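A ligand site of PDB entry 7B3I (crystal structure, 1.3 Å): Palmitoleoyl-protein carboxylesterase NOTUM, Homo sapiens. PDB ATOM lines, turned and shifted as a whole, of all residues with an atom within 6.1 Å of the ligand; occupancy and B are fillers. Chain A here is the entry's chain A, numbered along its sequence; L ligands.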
ATOM      1  N   GLY A  49      17.694  -3.871  13.908  1.00  0.00           N
ATOM      2  CA  GLY A  49      17.485  -2.447  13.813  1.00  0.00           C
ATOM      3  C   GLY A  49      17.409  -1.960  12.364  1.00  0.00           C
ATOM      4  O   GLY A  49      17.309  -2.735  11.414  1.00  0.00           O
ATOM      5  N   GLY A  50      17.453  -0.639  12.218  1.00  0.00           N
ATOM      6  CA  GLY A  50      17.377  -0.026  10.904  1.00  0.00           C
ATOM      7  C   GLY A  50      16.496   1.210  10.797  1.00  0.00           C
ATOM      8  O   GLY A  50      15.732   1.340   9.836  1.00  0.00           O
ATOM      9  N   TRP A  51      16.612   2.135  11.752  1.00  0.00           N
ATOM     10  CA  TRP A  51      15.891   3.426  11.724  1.00  0.00           C
ATOM     11  C   TRP A  51      14.382   3.167  11.717  1.00  0.00           C
ATOM     12  O   TRP A  51      13.906   2.296  12.452  1.00  0.00           O
ATOM     13  CB  TRP A  51      16.419   4.373  10.655  1.00  0.00           C
ATOM     14  CG  TRP A  51      17.822   4.750  10.920  1.00  0.00           C
ATOM     15  CD1 TRP A  51      18.942   4.132  10.448  1.00  0.00           C
ATOM     16  CD2 TRP A  51      18.273   5.811  11.757  1.00  0.00           C
ATOM     17  NE1 TRP A  51      20.068   4.761  10.925  1.00  0.00           N
ATOM     18  CE2 TRP A  51      19.685   5.803  11.730  1.00  0.00           C
ATOM     19  CE3 TRP A  51      17.625   6.788  12.512  1.00  0.00           C
ATOM     20  CZ2 TRP A  51      20.455   6.723  12.428  1.00  0.00           C
ATOM     21  CZ3 TRP A  51      18.394   7.714  13.203  1.00  0.00           C
ATOM     22  CH2 TRP A  51      19.790   7.669  13.161  1.00  0.00           C
ATOM     23  N   TYR A  52      13.615   3.927  10.923  1.00  0.00           N
ATOM     24  CA  TYR A  52      12.164   3.866  10.926  1.00  0.00           C
ATOM     25  C   TYR A  52      11.691   4.799   9.827  1.00  0.00           C
ATOM     26  O   TYR A  52      12.503   5.498   9.218  1.00  0.00           O
ATOM     27  CB  TYR A  52      11.572   4.316  12.273  1.00  0.00           C
ATOM     28  CG  TYR A  52      12.023   5.677  12.739  1.00  0.00           C
ATOM     29  CD1 TYR A  52      11.225   6.802  12.492  1.00  0.00           C
ATOM     30  CD2 TYR A  52      13.209   5.863  13.436  1.00  0.00           C
ATOM     31  CE1 TYR A  52      11.605   8.061  12.913  1.00  0.00           C
ATOM     32  CE2 TYR A  52      13.590   7.126  13.874  1.00  0.00           C
ATOM     33  CZ  TYR A  52      12.788   8.223  13.604  1.00  0.00           C
ATOM     34  OH  TYR A  52      13.168   9.482  14.025  1.00  0.00           O
ATOM     35  N   TYR A 105      13.486  -6.897  11.139  1.00  0.00           N
ATOM     36  CA  TYR A 105      12.780  -5.642  11.357  1.00  0.00           C
ATOM     37  C   TYR A 105      12.137  -5.234  10.046  1.00  0.00           C
ATOM     38  O   TYR A 105      12.829  -4.822   9.110  1.00  0.00           O
ATOM     39  CB  TYR A 105      13.809  -4.604  11.819  1.00  0.00           C
ATOM     40  CG  TYR A 105      13.294  -3.222  12.103  1.00  0.00           C
ATOM     41  CD1 TYR A 105      12.098  -3.013  12.802  1.00  0.00           C
ATOM     42  CD2 TYR A 105      14.048  -2.109  11.768  1.00  0.00           C
ATOM     43  CE1 TYR A 105      11.649  -1.715  13.094  1.00  0.00           C
ATOM     44  CE2 TYR A 105      13.633  -0.836  12.071  1.00  0.00           C
ATOM     45  CZ  TYR A 105      12.430  -0.642  12.732  1.00  0.00           C
ATOM     46  OH  TYR A 105      12.027   0.641  13.027  1.00  0.00           O
ATOM     47  N   VAL A 110      10.214   1.215  15.099  1.00  0.00           N
ATOM     48  CA  VAL A 110      11.030   1.004  16.300  1.00  0.00           C
ATOM     49  C   VAL A 110      10.362  -0.075  17.166  1.00  0.00           C
ATOM     50  O   VAL A 110      10.410  -0.049  18.407  1.00  0.00           O
ATOM     51  CB  VAL A 110      11.246   2.338  17.062  1.00  0.00           C
ATOM     52  CG1 VAL A 110      12.285   2.202  18.144  1.00  0.00           C
ATOM     53  CG2 VAL A 110      11.585   3.491  16.119  1.00  0.00           C
ATOM     54  N   SER A 154      19.574  -4.558  18.579  1.00  0.00           N
ATOM     55  CA  SER A 154      20.560  -3.516  18.292  1.00  0.00           C
ATOM     56  C   SER A 154      19.909  -2.334  17.594  1.00  0.00           C
ATOM     57  O   SER A 154      19.047  -2.502  16.719  1.00  0.00           O
ATOM     58  CB  SER A 154      21.688  -4.058  17.403  1.00  0.00           C
ATOM     59  OG  SER A 154      22.468  -5.040  18.097  1.00  0.00           O
ATOM     60  N   SER A 155      20.325  -1.129  17.974  1.00  0.00           N
ATOM     61  CA  SER A 155      19.908   0.126  17.313  1.00  0.00           C
ATOM     62  C   SER A 155      18.405   0.309  17.537  1.00  0.00           C
ATOM     63  O   SER A 155      17.971   0.300  18.695  1.00  0.00           O
ATOM     64  CB  SER A 155      20.367   0.129  15.864  1.00  0.00           C
ATOM     65  OG  SER A 155      21.780   0.143  15.801  1.00  0.00           O
ATOM     66  N   ALA A 156      17.598   0.487  16.493  1.00  0.00           N
ATOM     67  CA  ALA A 156      16.155   0.536  16.695  1.00  0.00           C
ATOM     68  C   ALA A 156      15.667  -0.714  17.415  1.00  0.00           C
ATOM     69  O   ALA A 156      14.685  -0.668  18.168  1.00  0.00           O
ATOM     70  CB  ALA A 156      15.421   0.683  15.354  1.00  0.00           C
ATOM     71  N   GLY A 157      16.337  -1.857  17.194  1.00  0.00           N
ATOM     72  CA  GLY A 157      16.002  -3.064  17.930  1.00  0.00           C
ATOM     73  C   GLY A 157      16.350  -2.986  19.402  1.00  0.00           C
ATOM     74  O   GLY A 157      15.682  -3.602  20.239  1.00  0.00           O
ATOM     75  N   THR A 159      16.214  -0.096  21.218  1.00  0.00           N
ATOM     76  CA  THR A 159      15.069   0.636  21.740  1.00  0.00           C
ATOM     77  C   THR A 159      13.832  -0.259  21.795  1.00  0.00           C
ATOM     78  O   THR A 159      13.064  -0.205  22.761  1.00  0.00           O
ATOM     79  CB  THR A 159      14.814   1.887  20.892  1.00  0.00           C
ATOM     80  OG1 THR A 159      16.049   2.594  20.729  1.00  0.00           O
ATOM     81  CG2 THR A 159      13.801   2.779  21.563  1.00  0.00           C
ATOM     82  N   SER A 188      22.891  -0.290  21.770  1.00  0.00           N
ATOM     83  CA  SER A 188      22.910   0.855  20.865  1.00  0.00           C
ATOM     84  C   SER A 188      21.522   1.432  20.640  1.00  0.00           C
ATOM     85  O   SER A 188      21.227   1.992  19.569  1.00  0.00           O
ATOM     86  CB  SER A 188      23.602   0.502  19.552  1.00  0.00           C
ATOM     87  OG  SER A 188      24.959   0.109  19.823  1.00  0.00           O
ATOM     88  N   GLY A 189      20.665   1.323  21.659  1.00  0.00           N
ATOM     89  CA  GLY A 189      19.345   1.900  21.592  1.00  0.00           C
ATOM     90  C   GLY A 189      19.043   2.881  22.702  1.00  0.00           C
ATOM     91  O   GLY A 189      17.869   3.171  22.958  1.00  0.00           O
ATOM     92  N   PHE A 191      19.505   6.507  23.719  1.00  0.00           N
ATOM     93  CA  PHE A 191      19.791   7.796  23.118  1.00  0.00           C
ATOM     94  C   PHE A 191      19.417   8.950  24.044  1.00  0.00           C
ATOM     95  O   PHE A 191      18.609   8.814  24.962  1.00  0.00           O
ATOM     96  CB  PHE A 191      19.031   7.932  21.787  1.00  0.00           C
ATOM     97  CG  PHE A 191      19.427   6.907  20.793  1.00  0.00           C
ATOM     98  CD1 PHE A 191      20.703   6.913  20.260  1.00  0.00           C
ATOM     99  CD2 PHE A 191      18.572   5.868  20.452  1.00  0.00           C
ATOM    100  CE1 PHE A 191      21.093   5.949  19.346  1.00  0.00           C
ATOM    101  CE2 PHE A 191      18.949   4.902  19.540  1.00  0.00           C
ATOM    102  CZ  PHE A 191      20.204   4.935  18.994  1.00  0.00           C
ATOM    103  N   ALA A 209      14.557  16.822  13.947  1.00  0.00           N
ATOM    104  CA  ALA A 209      15.132  16.137  15.102  1.00  0.00           C
ATOM    105  C   ALA A 209      14.329  14.903  15.438  1.00  0.00           C
ATOM    106  O   ALA A 209      13.118  14.858  15.201  1.00  0.00           O
ATOM    107  CB  ALA A 209      15.189  17.083  16.302  1.00  0.00           C
ATOM    108  N   PRO A 210      15.010  13.896  15.986  1.00  0.00           N
ATOM    109  CA  PRO A 210      14.334  12.659  16.398  1.00  0.00           C
ATOM    110  C   PRO A 210      13.041  12.840  17.188  1.00  0.00           C
ATOM    111  O   PRO A 210      12.052  12.184  16.858  1.00  0.00           O
ATOM    112  CB  PRO A 210      15.424  11.949  17.203  1.00  0.00           C
ATOM    113  CG  PRO A 210      16.667  12.354  16.525  1.00  0.00           C
ATOM    114  CD  PRO A 210      16.468  13.803  16.210  1.00  0.00           C
ATOM    115  N   THR A 211      13.016  13.702  18.214  1.00  0.00           N
ATOM    116  CA  THR A 211      11.822  13.790  19.050  1.00  0.00           C
ATOM    117  C   THR A 211      10.602  14.138  18.217  1.00  0.00           C
ATOM    118  O   THR A 211       9.503  13.618  18.456  1.00  0.00           O
ATOM    119  CB  THR A 211      11.977  14.808  20.183  1.00  0.00           C
ATOM    120  OG1 THR A 211      12.229  16.109  19.639  1.00  0.00           O
ATOM    121  CG2 THR A 211      13.099  14.407  21.126  1.00  0.00           C
ATOM    122  N   ILE A 214       9.760  11.052  15.863  1.00  0.00           N
ATOM    123  CA  ILE A 214       9.125  10.008  16.672  1.00  0.00           C
ATOM    124  C   ILE A 214       7.721  10.393  17.101  1.00  0.00           C
ATOM    125  O   ILE A 214       6.817   9.554  17.117  1.00  0.00           O
ATOM    126  CB  ILE A 214       9.995   9.577  17.872  1.00  0.00           C
ATOM    127  CG1 ILE A 214      11.190   8.751  17.419  1.00  0.00           C
ATOM    128  CG2 ILE A 214       9.179   8.774  18.888  1.00  0.00           C
ATOM    129  CD1 ILE A 214      10.852   7.654  16.446  1.00  0.00           C
ATOM    130  N   PHE A 242      10.612   6.509  24.324  1.00  0.00           N
ATOM    131  CA  PHE A 242      11.610   5.997  23.394  1.00  0.00           C
ATOM    132  C   PHE A 242      13.028   6.321  23.839  1.00  0.00           C
ATOM    133  O   PHE A 242      13.978   5.862  23.206  1.00  0.00           O
ATOM    134  CB  PHE A 242      11.355   6.576  21.997  1.00  0.00           C
ATOM    135  CG  PHE A 242      10.251   5.886  21.250  1.00  0.00           C
ATOM    136  CD1 PHE A 242       8.948   5.925  21.707  1.00  0.00           C
ATOM    137  CD2 PHE A 242      10.499   5.305  20.002  1.00  0.00           C
ATOM    138  CE1 PHE A 242       7.915   5.296  20.996  1.00  0.00           C
ATOM    139  CE2 PHE A 242       9.475   4.702  19.284  1.00  0.00           C
ATOM    140  CZ  PHE A 242       8.190   4.699  19.781  1.00  0.00           C
ATOM    141  N   PHE A 243      13.180   7.092  24.907  1.00  0.00           N
ATOM    142  CA  PHE A 243      14.489   7.475  25.399  1.00  0.00           C
ATOM    143  C   PHE A 243      14.832   6.625  26.611  1.00  0.00           C
ATOM    144  O   PHE A 243      14.150   6.700  27.629  1.00  0.00           O
ATOM    145  CB  PHE A 243      14.528   8.973  25.673  1.00  0.00           C
ATOM    146  CG  PHE A 243      14.540   9.751  24.400  1.00  0.00           C
ATOM    147  CD1 PHE A 243      15.746  10.020  23.775  1.00  0.00           C
ATOM    148  CD2 PHE A 243      13.356  10.035  23.731  1.00  0.00           C
ATOM    149  CE1 PHE A 243      15.780  10.655  22.548  1.00  0.00           C
ATOM    150  CE2 PHE A 243      13.375  10.674  22.498  1.00  0.00           C
ATOM    151  CZ  PHE A 243      14.590  10.987  21.909  1.00  0.00           C
ATOM    152  N   ASP A 263      28.123   7.212  20.456  1.00  0.00           N
ATOM    153  CA  ASP A 263      27.455   6.409  19.447  1.00  0.00           C
ATOM    154  C   ASP A 263      27.326   7.200  18.150  1.00  0.00           C
ATOM    155  O   ASP A 263      26.907   8.357  18.167  1.00  0.00           O
ATOM    156  CB  ASP A 263      26.078   6.014  19.977  1.00  0.00           C
ATOM    157  CG  ASP A 263      25.323   5.159  19.036  1.00  0.00           C
ATOM    158  OD1 ASP A 263      25.439   3.927  19.116  1.00  0.00           O
ATOM    159  OD2 ASP A 263      24.610   5.722  18.182  1.00  0.00           O
ATOM    160  N   ALA A 265      25.225   6.985  15.708  1.00  0.00           N
ATOM    161  CA  ALA A 265      23.882   7.430  15.359  1.00  0.00           C
ATOM    162  C   ALA A 265      23.466   8.626  16.210  1.00  0.00           C
ATOM    163  O   ALA A 265      22.791   9.545  15.720  1.00  0.00           O
ATOM    164  CB  ALA A 265      22.873   6.291  15.474  1.00  0.00           C
ATOM    165  N   GLN A 266      23.864   8.644  17.488  1.00  0.00           N
ATOM    166  CA  GLN A 266      23.645   9.818  18.316  1.00  0.00           C
ATOM    167  C   GLN A 266      24.348  11.039  17.724  1.00  0.00           C
ATOM    168  O   GLN A 266      23.775  12.128  17.623  1.00  0.00           O
ATOM    169  CB  GLN A 266      24.177   9.545  19.728  1.00  0.00           C
ATOM    170  CG  GLN A 266      24.030  10.725  20.679  1.00  0.00           C
ATOM    171  CD  GLN A 266      22.604  10.867  21.185  1.00  0.00           C
ATOM    172  OE1 GLN A 266      22.012   9.906  21.682  1.00  0.00           O
ATOM    173  NE2 GLN A 266      22.060  12.072  21.097  1.00  0.00           N
ATOM    174  N   VAL A 269      22.440  12.328  14.510  1.00  0.00           N
ATOM    175  CA  VAL A 269      21.255  13.146  14.768  1.00  0.00           C
ATOM    176  C   VAL A 269      21.660  14.468  15.411  1.00  0.00           C
ATOM    177  O   VAL A 269      20.984  15.491  15.210  1.00  0.00           O
ATOM    178  CB  VAL A 269      20.186  12.387  15.571  1.00  0.00           C
ATOM    179  CG1 VAL A 269      19.753  11.110  14.852  1.00  0.00           C
ATOM    180  CG2 VAL A 269      20.657  12.095  17.006  1.00  0.00           C
ATOM    181  N   HIS A 312      29.110   1.968  16.565  1.00  0.00           N
ATOM    182  CA  HIS A 312      27.677   1.746  16.506  1.00  0.00           C
ATOM    183  C   HIS A 312      27.415   0.244  16.451  1.00  0.00           C
ATOM    184  O   HIS A 312      27.991  -0.442  15.615  1.00  0.00           O
ATOM    185  CB  HIS A 312      27.060   2.437  15.285  1.00  0.00           C
ATOM    186  CG  HIS A 312      25.565   2.367  15.250  1.00  0.00           C
ATOM    187  ND1 HIS A 312      24.772   2.853  16.271  1.00  0.00           N
ATOM    188  CD2 HIS A 312      24.718   1.864  14.326  1.00  0.00           C
ATOM    189  CE1 HIS A 312      23.508   2.650  15.978  1.00  0.00           C
ATOM    190  NE2 HIS A 312      23.439   2.054  14.800  1.00  0.00           N
ATOM    191  N   GLU A 313      26.569  -0.235  17.365  1.00  0.00           N
ATOM    192  CA  GLU A 313      26.219  -1.648  17.540  1.00  0.00           C
ATOM    193  C   GLU A 313      27.402  -2.461  18.035  1.00  0.00           C
ATOM    194  O   GLU A 313      28.553  -2.040  17.873  1.00  0.00           O
ATOM    195  CB  GLU A 313      25.601  -2.230  16.256  1.00  0.00           C
ATOM    196  CG  GLU A 313      24.307  -1.564  15.846  1.00  0.00           C
ATOM    197  CD  GLU A 313      23.676  -2.150  14.588  1.00  0.00           C
ATOM    198  OE1 GLU A 313      22.460  -1.989  14.395  1.00  0.00           O
ATOM    199  OE2 GLU A 313      24.413  -2.764  13.778  1.00  0.00           O
HETATM  200  C1  LIG L   1      14.396   8.008  18.754  1.00  0.00           C
HETATM  201  C2  LIG L   1      14.672   7.541  20.016  1.00  0.00           C
HETATM  202  C3  LIG L   1      15.059   6.235  20.185  1.00  0.00           C
HETATM  203  C4  LIG L   1      15.184   5.397  19.092  1.00  0.00           C
HETATM  204  C5  LIG L   1      14.889   5.885  17.825  1.00  0.00           C
HETATM  205  C6  LIG L   1      14.494   7.191  17.644  1.00  0.00           C
HETATM  206  C7  LIG L   1      16.765   4.805  15.946  1.00  0.00           C
HETATM  207  C8  LIG L   1      19.058   2.629  14.077  1.00  0.00           C
HETATM  208  C9  LIG L   1      19.370   4.640  15.118  1.00  0.00           C
HETATM  209  C10 LIG L   1      18.991   5.755  15.852  1.00  0.00           C
HETATM  210  C11 LIG L   1      17.674   5.860  16.275  1.00  0.00           C
HETATM  211  N1  LIG L   1      17.148   3.758  15.243  1.00  0.00           N
HETATM  212  N2  LIG L   1      18.454   3.688  14.853  1.00  0.00           N
HETATM  213  N3  LIG L   1      20.412   2.954  13.881  1.00  0.00           N
HETATM  214  N4  LIG L   1      20.647   4.177  14.504  1.00  0.00           N
HETATM  215  O1  LIG L   1      18.453   1.677  13.729  1.00  0.00           O
HETATM  216  S1  LIG L   1      15.041   4.787  16.408  1.00  0.00           S
HETATM  217 CL1  LIG L   1      13.878   9.697  18.541  1.00  0.00          CL
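The backbone NH (N) of Ala 156 lies within hydrogen-bond range of an oxygen (O1) of the ligand (3.1 Å). A nitrogen (N3) of the ligand lies within hydrogen-bond range of a ring nitrogen (NE2) of His 312 (3.3 Å). An oxygen (O1) of the ligand is in hydrogen-bond range of the backbone NH (N) of Trp 51 (2.7 Å). N of Gly 50 is in hydrogen-bond range of O1 of the ligand (2.9 Å).
The side-chain hydroxyl of Tyr 105 sits at hydrogen-bond distance from the backbone carbonyl oxygen of Trp 51. OG of Ser 155 lies within hydrogen-bond range of OE1 of Glu 313, 2.6 Å away. A ring nitrogen (ND1) of His 312 is in hydrogen-bond range of the side-chain carboxylate of Asp 263 (3.1 Å). The side-chain carboxylate (OD2) of Asp 263 is in hydrogen-bond range of the backbone NH (N) of Ala 265, at 2.8 Å. The side-chain hydroxyl (OG) of Ser 155 sits at hydrogen-bond distance from a ring nitrogen (NE2) of His 312, at 2.7 Å. The side-chain hydroxyl of Tyr 105 is in hydrogen-bond range of the backbone NH of Val 110, at 2.8 Å. The backbone carbonyl oxygen of Gly 189 lies within hydrogen-bond range of the side-chain hydroxyl of Thr 159, 2.9 Å away.
Merely in contact with the ligand: Tyr 52, Val 110, Ser 155, Thr 159, Phe 191, Pro 210, Ile 214, Phe 242, Phe 243 and Ala 265. Hydrophobic or aromatic side chains that line the ligand: Trp 51, Tyr 52, Val 110, Ala 156, Phe 191, Pro 210, Ile 214, Phe 242, Phe 243, Ala 265 and His 312. Within 4 Å of the ligand: Gly 50, Trp 51, Tyr 52, Val 110, Ser 155, Ala 156, Thr 159, Phe 191, Pro 210, Ile 214, Phe 242, Phe 243, Ala 265 and His 312. The nearest printed residue that does not touch the ligand is Gly 49 (4.02 Å).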
